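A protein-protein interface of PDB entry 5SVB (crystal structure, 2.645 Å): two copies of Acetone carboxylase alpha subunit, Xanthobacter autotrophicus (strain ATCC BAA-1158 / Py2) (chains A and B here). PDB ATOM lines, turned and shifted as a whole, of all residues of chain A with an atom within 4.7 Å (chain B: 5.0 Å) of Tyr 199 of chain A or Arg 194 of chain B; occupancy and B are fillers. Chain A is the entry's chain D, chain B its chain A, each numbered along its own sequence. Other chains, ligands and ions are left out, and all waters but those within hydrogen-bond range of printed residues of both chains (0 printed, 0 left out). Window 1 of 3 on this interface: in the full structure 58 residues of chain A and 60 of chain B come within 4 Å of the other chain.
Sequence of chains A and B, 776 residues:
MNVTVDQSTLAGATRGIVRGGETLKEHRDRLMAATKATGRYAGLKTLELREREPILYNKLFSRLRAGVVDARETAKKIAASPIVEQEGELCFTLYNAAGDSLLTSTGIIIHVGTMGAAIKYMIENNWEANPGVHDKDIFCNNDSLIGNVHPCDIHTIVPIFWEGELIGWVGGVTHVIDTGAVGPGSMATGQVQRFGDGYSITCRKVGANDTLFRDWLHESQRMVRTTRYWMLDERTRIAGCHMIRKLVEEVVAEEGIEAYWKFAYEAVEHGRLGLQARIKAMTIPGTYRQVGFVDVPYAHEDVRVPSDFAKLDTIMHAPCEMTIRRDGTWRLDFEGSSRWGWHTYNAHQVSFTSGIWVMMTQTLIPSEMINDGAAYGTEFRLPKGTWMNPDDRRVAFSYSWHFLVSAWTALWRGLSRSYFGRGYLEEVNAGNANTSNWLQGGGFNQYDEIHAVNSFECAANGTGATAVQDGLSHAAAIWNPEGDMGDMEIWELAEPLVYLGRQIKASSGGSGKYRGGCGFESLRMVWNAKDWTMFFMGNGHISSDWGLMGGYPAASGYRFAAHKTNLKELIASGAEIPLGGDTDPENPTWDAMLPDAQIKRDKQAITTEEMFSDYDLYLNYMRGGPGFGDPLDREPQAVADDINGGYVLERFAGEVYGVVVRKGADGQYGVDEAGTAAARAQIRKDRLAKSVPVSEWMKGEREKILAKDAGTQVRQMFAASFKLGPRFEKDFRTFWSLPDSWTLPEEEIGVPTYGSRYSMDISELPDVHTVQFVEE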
ATOM      1  N   ASN A 142     -31.953  31.009  16.990  1.00  0.00           N
ATOM      2  CA  ASN A 142     -31.545  30.125  15.904  1.00  0.00           C
ATOM      3  C   ASN A 142     -31.790  28.670  16.281  1.00  0.00           C
ATOM      4  O   ASN A 142     -31.125  27.771  15.756  1.00  0.00           O
ATOM      5  CB  ASN A 142     -30.068  30.324  15.554  1.00  0.00           C
ATOM      6  CG  ASN A 142     -29.140  29.738  16.598  1.00  0.00           C
ATOM      7  OD1 ASN A 142     -29.468  29.699  17.782  1.00  0.00           O
ATOM      8  ND2 ASN A 142     -27.979  29.270  16.162  1.00  0.00           N
ATOM      9  N   SER A 144     -32.315  24.875  17.320  1.00  0.00           N
ATOM     10  CA  SER A 144     -32.379  23.658  16.520  1.00  0.00           C
ATOM     11  C   SER A 144     -33.735  22.980  16.649  1.00  0.00           C
ATOM     12  O   SER A 144     -34.264  22.444  15.669  1.00  0.00           O
ATOM     13  CB  SER A 144     -31.271  22.699  16.953  1.00  0.00           C
ATOM     14  OG  SER A 144     -29.995  23.309  16.852  1.00  0.00           O
ATOM     15  N   GLY A 180     -19.065  28.741  13.950  1.00  0.00           N
ATOM     16  CA  GLY A 180     -18.466  27.435  14.154  1.00  0.00           C
ATOM     17  C   GLY A 180     -19.350  26.309  13.653  1.00  0.00           C
ATOM     18  O   GLY A 180     -18.934  25.151  13.607  1.00  0.00           O
ATOM     19  N   TYR A 199     -24.054  25.367  18.094  1.00  0.00           N
ATOM     20  CA  TYR A 199     -24.590  26.399  18.971  1.00  0.00           C
ATOM     21  C   TYR A 199     -26.117  26.463  18.904  1.00  0.00           C
ATOM     22  O   TYR A 199     -26.748  25.933  17.985  1.00  0.00           O
ATOM     23  CB  TYR A 199     -23.995  27.762  18.616  1.00  0.00           C
ATOM     24  CG  TYR A 199     -22.503  27.860  18.849  1.00  0.00           C
ATOM     25  CD1 TYR A 199     -21.999  28.223  20.093  1.00  0.00           C
ATOM     26  CD2 TYR A 199     -21.604  27.589  17.828  1.00  0.00           C
ATOM     27  CE1 TYR A 199     -20.637  28.313  20.310  1.00  0.00           C
ATOM     28  CE2 TYR A 199     -20.239  27.677  18.037  1.00  0.00           C
ATOM     29  CZ  TYR A 199     -19.762  28.039  19.279  1.00  0.00           C
ATOM     30  OH  TYR A 199     -18.406  28.130  19.493  1.00  0.00           O
ATOM     31  N   SER A 200     -26.698  27.161  19.882  1.00  0.00           N
ATOM     32  CA  SER A 200     -28.150  27.177  20.066  1.00  0.00           C
ATOM     33  C   SER A 200     -28.584  28.421  20.831  1.00  0.00           C
ATOM     34  O   SER A 200     -28.120  28.654  21.955  1.00  0.00           O
ATOM     35  CB  SER A 200     -28.596  25.924  20.820  1.00  0.00           C
ATOM     36  OG  SER A 200     -30.002  25.781  20.792  1.00  0.00           O
ATOM     37  N   ILE A 201     -29.501  29.193  20.246  1.00  0.00           N
ATOM     38  CA  ILE A 201     -30.100  30.375  20.867  1.00  0.00           C
ATOM     39  C   ILE A 201     -31.612  30.182  20.846  1.00  0.00           C
ATOM     40  O   ILE A 201     -32.209  30.064  19.769  1.00  0.00           O
ATOM     41  CB  ILE A 201     -29.719  31.671  20.131  1.00  0.00           C
ATOM     42  CG1 ILE A 201     -28.204  31.770  19.928  1.00  0.00           C
ATOM     43  CG2 ILE A 201     -30.216  32.886  20.902  1.00  0.00           C
ATOM     44  CD1 ILE A 201     -27.812  32.664  18.774  1.00  0.00           C
ATOM     45  N   ARG A 222     -17.757  35.033  21.024  1.00  0.00           N
ATOM     46  CA  ARG A 222     -17.013  33.794  21.195  1.00  0.00           C
ATOM     47  C   ARG A 222     -17.601  32.650  20.383  1.00  0.00           C
ATOM     48  O   ARG A 222     -16.930  31.628  20.200  1.00  0.00           O
ATOM     49  CB  ARG A 222     -16.979  33.403  22.676  1.00  0.00           C
ATOM     50  CG  ARG A 222     -16.100  34.302  23.528  1.00  0.00           C
ATOM     51  CD  ARG A 222     -16.508  34.257  24.988  1.00  0.00           C
ATOM     52  NE  ARG A 222     -15.471  34.801  25.862  1.00  0.00           N
ATOM     53  CZ  ARG A 222     -15.180  36.092  25.968  1.00  0.00           C
ATOM     54  NH1 ARG A 222     -15.838  36.989  25.247  1.00  0.00           N
ATOM     55  NH2 ARG A 222     -14.221  36.490  26.791  1.00  0.00           N
ATOM     56  N   MET A 223     -18.825  32.805  19.887  1.00  0.00           N
ATOM     57  CA  MET A 223     -19.467  31.792  19.056  1.00  0.00           C
ATOM     58  C   MET A 223     -18.998  31.870  17.611  1.00  0.00           C
ATOM     59  O   MET A 223     -19.598  31.255  16.731  1.00  0.00           O
ATOM     60  CB  MET A 223     -20.988  31.966  19.081  1.00  0.00           C
ATOM     61  CG  MET A 223     -21.653  31.772  20.427  1.00  0.00           C
ATOM     62  SD  MET A 223     -23.556  32.179  20.284  1.00  0.00           S
ATOM     63  CE  MET A 223     -23.988  32.384  22.172  1.00  0.00           C
ATOM     64  N   ASP B 143     -17.036  30.171  30.777  1.00  0.00           N
ATOM     65  CA  ASP B 143     -16.360  30.571  29.551  1.00  0.00           C
ATOM     66  C   ASP B 143     -14.967  29.964  29.453  1.00  0.00           C
ATOM     67  O   ASP B 143     -14.221  29.903  30.434  1.00  0.00           O
ATOM     68  CB  ASP B 143     -16.273  32.096  29.482  1.00  0.00           C
ATOM     69  CG  ASP B 143     -15.846  32.596  28.119  1.00  0.00           C
ATOM     70  OD1 ASP B 143     -16.112  31.899  27.119  1.00  0.00           O
ATOM     71  OD2 ASP B 143     -15.248  33.688  28.043  1.00  0.00           O
ATOM     72  N   SER B 144     -14.615  29.525  28.245  1.00  0.00           N
ATOM     73  CA  SER B 144     -13.304  28.938  28.006  1.00  0.00           C
ATOM     74  C   SER B 144     -12.215  30.002  27.924  1.00  0.00           C
ATOM     75  O   SER B 144     -11.083  29.767  28.363  1.00  0.00           O
ATOM     76  CB  SER B 144     -13.334  28.113  26.720  1.00  0.00           C
ATOM     77  OG  SER B 144     -13.887  28.861  25.653  1.00  0.00           O
ATOM     78  N   LEU B 145     -12.530  31.170  27.363  1.00  0.00           N
ATOM     79  CA  LEU B 145     -11.521  32.215  27.224  1.00  0.00           C
ATOM     80  C   LEU B 145     -11.219  32.903  28.548  1.00  0.00           C
ATOM     81  O   LEU B 145     -10.078  33.322  28.774  1.00  0.00           O
ATOM     82  CB  LEU B 145     -11.967  33.247  26.185  1.00  0.00           C
ATOM     83  CG  LEU B 145     -12.303  32.716  24.787  1.00  0.00           C
ATOM     84  CD1 LEU B 145     -12.206  33.841  23.765  1.00  0.00           C
ATOM     85  CD2 LEU B 145     -11.414  31.545  24.376  1.00  0.00           C
ATOM     86  N   GLN B 191     -12.577  15.517  19.380  1.00  0.00           N
ATOM     87  CA  GLN B 191     -12.414  16.946  19.165  1.00  0.00           C
ATOM     88  C   GLN B 191     -10.946  17.301  18.953  1.00  0.00           C
ATOM     89  O   GLN B 191     -10.040  16.662  19.493  1.00  0.00           O
ATOM     90  CB  GLN B 191     -12.971  17.731  20.353  1.00  0.00           C
ATOM     91  CG  GLN B 191     -12.942  19.238  20.151  1.00  0.00           C
ATOM     92  CD  GLN B 191     -13.564  20.001  21.300  1.00  0.00           C
ATOM     93  OE1 GLN B 191     -13.650  19.500  22.421  1.00  0.00           O
ATOM     94  NE2 GLN B 191     -14.001  21.224  21.026  1.00  0.00           N
ATOM     95  N   VAL B 192     -10.722  18.339  18.150  1.00  0.00           N
ATOM     96  CA  VAL B 192      -9.379  18.852  17.897  1.00  0.00           C
ATOM     97  C   VAL B 192      -9.262  20.346  18.107  1.00  0.00           C
ATOM     98  O   VAL B 192      -8.136  20.854  18.269  1.00  0.00           O
ATOM     99  CB  VAL B 192      -8.934  18.495  16.466  1.00  0.00           C
ATOM    100  CG1 VAL B 192      -8.815  17.031  16.326  1.00  0.00           C
ATOM    101  CG2 VAL B 192      -9.926  19.045  15.442  1.00  0.00           C
ATOM    102  N   GLN B 193     -10.358  21.096  18.086  1.00  0.00           N
ATOM    103  CA  GLN B 193     -10.300  22.540  18.224  1.00  0.00           C
ATOM    104  C   GLN B 193     -11.650  23.036  18.709  1.00  0.00           C
ATOM    105  O   GLN B 193     -12.684  22.413  18.457  1.00  0.00           O
ATOM    106  CB  GLN B 193      -9.919  23.211  16.900  1.00  0.00           C
ATOM    107  CG  GLN B 193     -10.926  23.010  15.789  1.00  0.00           C
ATOM    108  CD  GLN B 193     -10.385  23.433  14.438  1.00  0.00           C
ATOM    109  OE1 GLN B 193     -10.213  24.622  14.171  1.00  0.00           O
ATOM    110  NE2 GLN B 193     -10.108  22.458  13.581  1.00  0.00           N
ATOM    111  N   ARG B 194     -11.624  24.162  19.407  1.00  0.00           N
ATOM    112  CA  ARG B 194     -12.817  24.732  20.011  1.00  0.00           C
ATOM    113  C   ARG B 194     -13.535  25.663  19.042  1.00  0.00           C
ATOM    114  O   ARG B 194     -14.454  25.250  18.333  1.00  0.00           O
ATOM    115  CB  ARG B 194     -12.431  25.472  21.291  1.00  0.00           C
ATOM    116  CG  ARG B 194     -13.528  26.321  21.907  1.00  0.00           C
ATOM    117  CD  ARG B 194     -13.344  27.796  21.587  1.00  0.00           C
ATOM    118  NE  ARG B 194     -13.944  28.645  22.609  1.00  0.00           N
ATOM    119  CZ  ARG B 194     -15.243  28.908  22.704  1.00  0.00           C
ATOM    120  NH1 ARG B 194     -15.690  29.692  23.673  1.00  0.00           N
ATOM    121  NH2 ARG B 194     -16.098  28.386  21.834  1.00  0.00           N
ATOM    122  N   TYR B 199     -19.821  25.172  23.842  1.00  0.00           N
ATOM    123  CA  TYR B 199     -20.713  25.654  24.891  1.00  0.00           C
ATOM    124  C   TYR B 199     -19.993  26.670  25.766  1.00  0.00           C
ATOM    125  O   TYR B 199     -19.144  26.305  26.576  1.00  0.00           O
ATOM    126  CB  TYR B 199     -21.218  24.495  25.750  1.00  0.00           C
ATOM    127  CG  TYR B 199     -21.883  23.382  24.971  1.00  0.00           C
ATOM    128  CD1 TYR B 199     -22.338  23.580  23.673  1.00  0.00           C
ATOM    129  CD2 TYR B 199     -22.058  22.131  25.539  1.00  0.00           C
ATOM    130  CE1 TYR B 199     -22.946  22.559  22.965  1.00  0.00           C
ATOM    131  CE2 TYR B 199     -22.663  21.111  24.841  1.00  0.00           C
ATOM    132  CZ  TYR B 199     -23.105  21.326  23.556  1.00  0.00           C
ATOM    133  OH  TYR B 199     -23.710  20.304  22.862  1.00  0.00           O
ATOM    134  N   SER B 200     -20.341  27.944  25.608  1.00  0.00           N
ATOM    135  CA  SER B 200     -19.662  29.029  26.306  1.00  0.00           C
ATOM    136  C   SER B 200     -20.695  29.965  26.910  1.00  0.00           C
ATOM    137  O   SER B 200     -21.542  30.507  26.193  1.00  0.00           O
ATOM    138  CB  SER B 200     -18.733  29.793  25.360  1.00  0.00           C
ATOM    139  OG  SER B 200     -17.977  30.761  26.063  1.00  0.00           O
ATOM    140  N   ARG B 393      -7.651  31.012  19.889  1.00  0.00           N
ATOM    141  CA  ARG B 393      -9.060  30.718  20.135  1.00  0.00           C
ATOM    142  C   ARG B 393      -9.472  29.343  19.628  1.00  0.00           C
ATOM    143  O   ARG B 393     -10.513  28.831  20.051  1.00  0.00           O
ATOM    144  CB  ARG B 393      -9.959  31.772  19.492  1.00  0.00           C
ATOM    145  CG  ARG B 393      -9.381  33.184  19.476  1.00  0.00           C
ATOM    146  CD  ARG B 393     -10.426  34.252  19.783  1.00  0.00           C
ATOM    147  NE  ARG B 393     -10.968  34.879  18.580  1.00  0.00           N
ATOM    148  CZ  ARG B 393     -12.077  34.497  17.954  1.00  0.00           C
ATOM    149  NH1 ARG B 393     -12.791  33.471  18.401  1.00  0.00           N
ATOM    150  NH2 ARG B 393     -12.476  35.146  16.868  1.00  0.00           N
ATOM    151  N   ARG B 394      -8.693  28.741  18.727  1.00  0.00           N
ATOM    152  CA  ARG B 394      -9.031  27.422  18.209  1.00  0.00           C
ATOM    153  C   ARG B 394      -8.834  26.317  19.239  1.00  0.00           C
ATOM    154  O   ARG B 394      -9.419  25.240  19.091  1.00  0.00           O
ATOM    155  CB  ARG B 394      -8.181  27.111  16.975  1.00  0.00           C
ATOM    156  CG  ARG B 394      -8.515  27.940  15.749  1.00  0.00           C
ATOM    157  CD  ARG B 394      -7.531  27.679  14.621  1.00  0.00           C
ATOM    158  NE  ARG B 394      -6.200  28.189  14.934  1.00  0.00           N
ATOM    159  CZ  ARG B 394      -5.147  28.088  14.129  1.00  0.00           C
ATOM    160  NH1 ARG B 394      -5.256  27.491  12.949  1.00  0.00           N
ATOM    161  NH2 ARG B 394      -3.978  28.586  14.507  1.00  0.00           N
ATOM    162  N   VAL B 395      -8.037  26.557  20.280  1.00  0.00           N
ATOM    163  CA  VAL B 395      -7.591  25.476  21.150  1.00  0.00           C
ATOM    164  C   VAL B 395      -8.758  24.931  21.960  1.00  0.00           C
ATOM    165  O   VAL B 395      -9.637  25.679  22.408  1.00  0.00           O
ATOM    166  CB  VAL B 395      -6.463  25.967  22.073  1.00  0.00           C
ATOM    167  CG1 VAL B 395      -5.918  24.819  22.897  1.00  0.00           C
ATOM    168  CG2 VAL B 395      -5.355  26.604  21.261  1.00  0.00           C
ATOM    169  N   ALA B 396      -8.762  23.617  22.162  1.00  0.00           N
ATOM    170  CA  ALA B 396      -9.739  22.936  22.998  1.00  0.00           C
ATOM    171  C   ALA B 396      -9.137  22.594  24.358  1.00  0.00           C
ATOM    172  O   ALA B 396      -7.922  22.439  24.509  1.00  0.00           O
ATOM    173  CB  ALA B 396     -10.239  21.661  22.316  1.00  0.00           C
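The guanidinium group of Arg 222 of chain A lies within salt-bridge range of the side-chain carboxylate of Asp 143 of chain B (2.5 Å).
NH2 of Arg 194 of chain B is in hydrogen-bond range of OH of Tyr 199 of chain A, 3.3 Å away.
The side-chain carboxylate of Asp 143 of chain B lies within hydrogen-bond range of the side-chain hydroxyl of Ser 200 of chain B, 2.4 Å away.
The guanidinium group of Arg 194 of chain B sits at hydrogen-bond distance from the side-chain hydroxyl of Ser 144 of chain B (2.8 Å).
The side-chain hydroxyl (OG) of Ser 200 of chain B is in hydrogen-bond range of the guanidinium group (NH1) of Arg 194 of chain B (3.5 Å).
The backbone NH of Arg 194 of chain B lies within hydrogen-bond range of the backbone carbonyl oxygen of Arg 394 of chain B.
Among the printed residues, pairs that only touch across the chains: Arg 222 of chain A with Leu 145 of chain B, Arg 222 of chain A with Arg 194 of chain B and Arg 222 of chain A with Ser 200 of chain B.
Tyr 199 of chain A touches one residue of chain B.
Printed residues of chain A within 4 Å of Arg 194 of chain B: Tyr 199 (3.3 Å) and Arg 222 (3.7 Å).
Of the printed residues of chain A, Ser 200 of chain B touches Arg 222 (3.9 Å).
Printed residues of chain A within 4 Å of Asp 143 of chain B: Arg 222 (2.5 Å).
Ala 396 of chain B touches none of the printed residues of chain A.
Gly 180 of chain A touches none of the printed residues of chain B.
The nearest residue of chain B that does not touch Tyr 199 of chain A is Tyr 199 of chain B (4.8 Å).
Printed residues of chain B that touch a printed residue of chain A: Asp 143, Leu 145, Arg 194 and Ser 200.
Hydrophobic or aromatic side chains of chain B that line the printed part of chain A: Leu 145.
Among the printed residues, Asp or Glu carboxylates within 4 Å of a Lys or Arg side-chain nitrogen of the other chain: Arg 222 of chain A with Asp 143 of chain B (2.5 Å).
Positions printed for both chains: 144, 199 and 200.
Of the 5 pairs that touch across the chains among the printed residues, none has its exchanged pair printed and touching as well.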
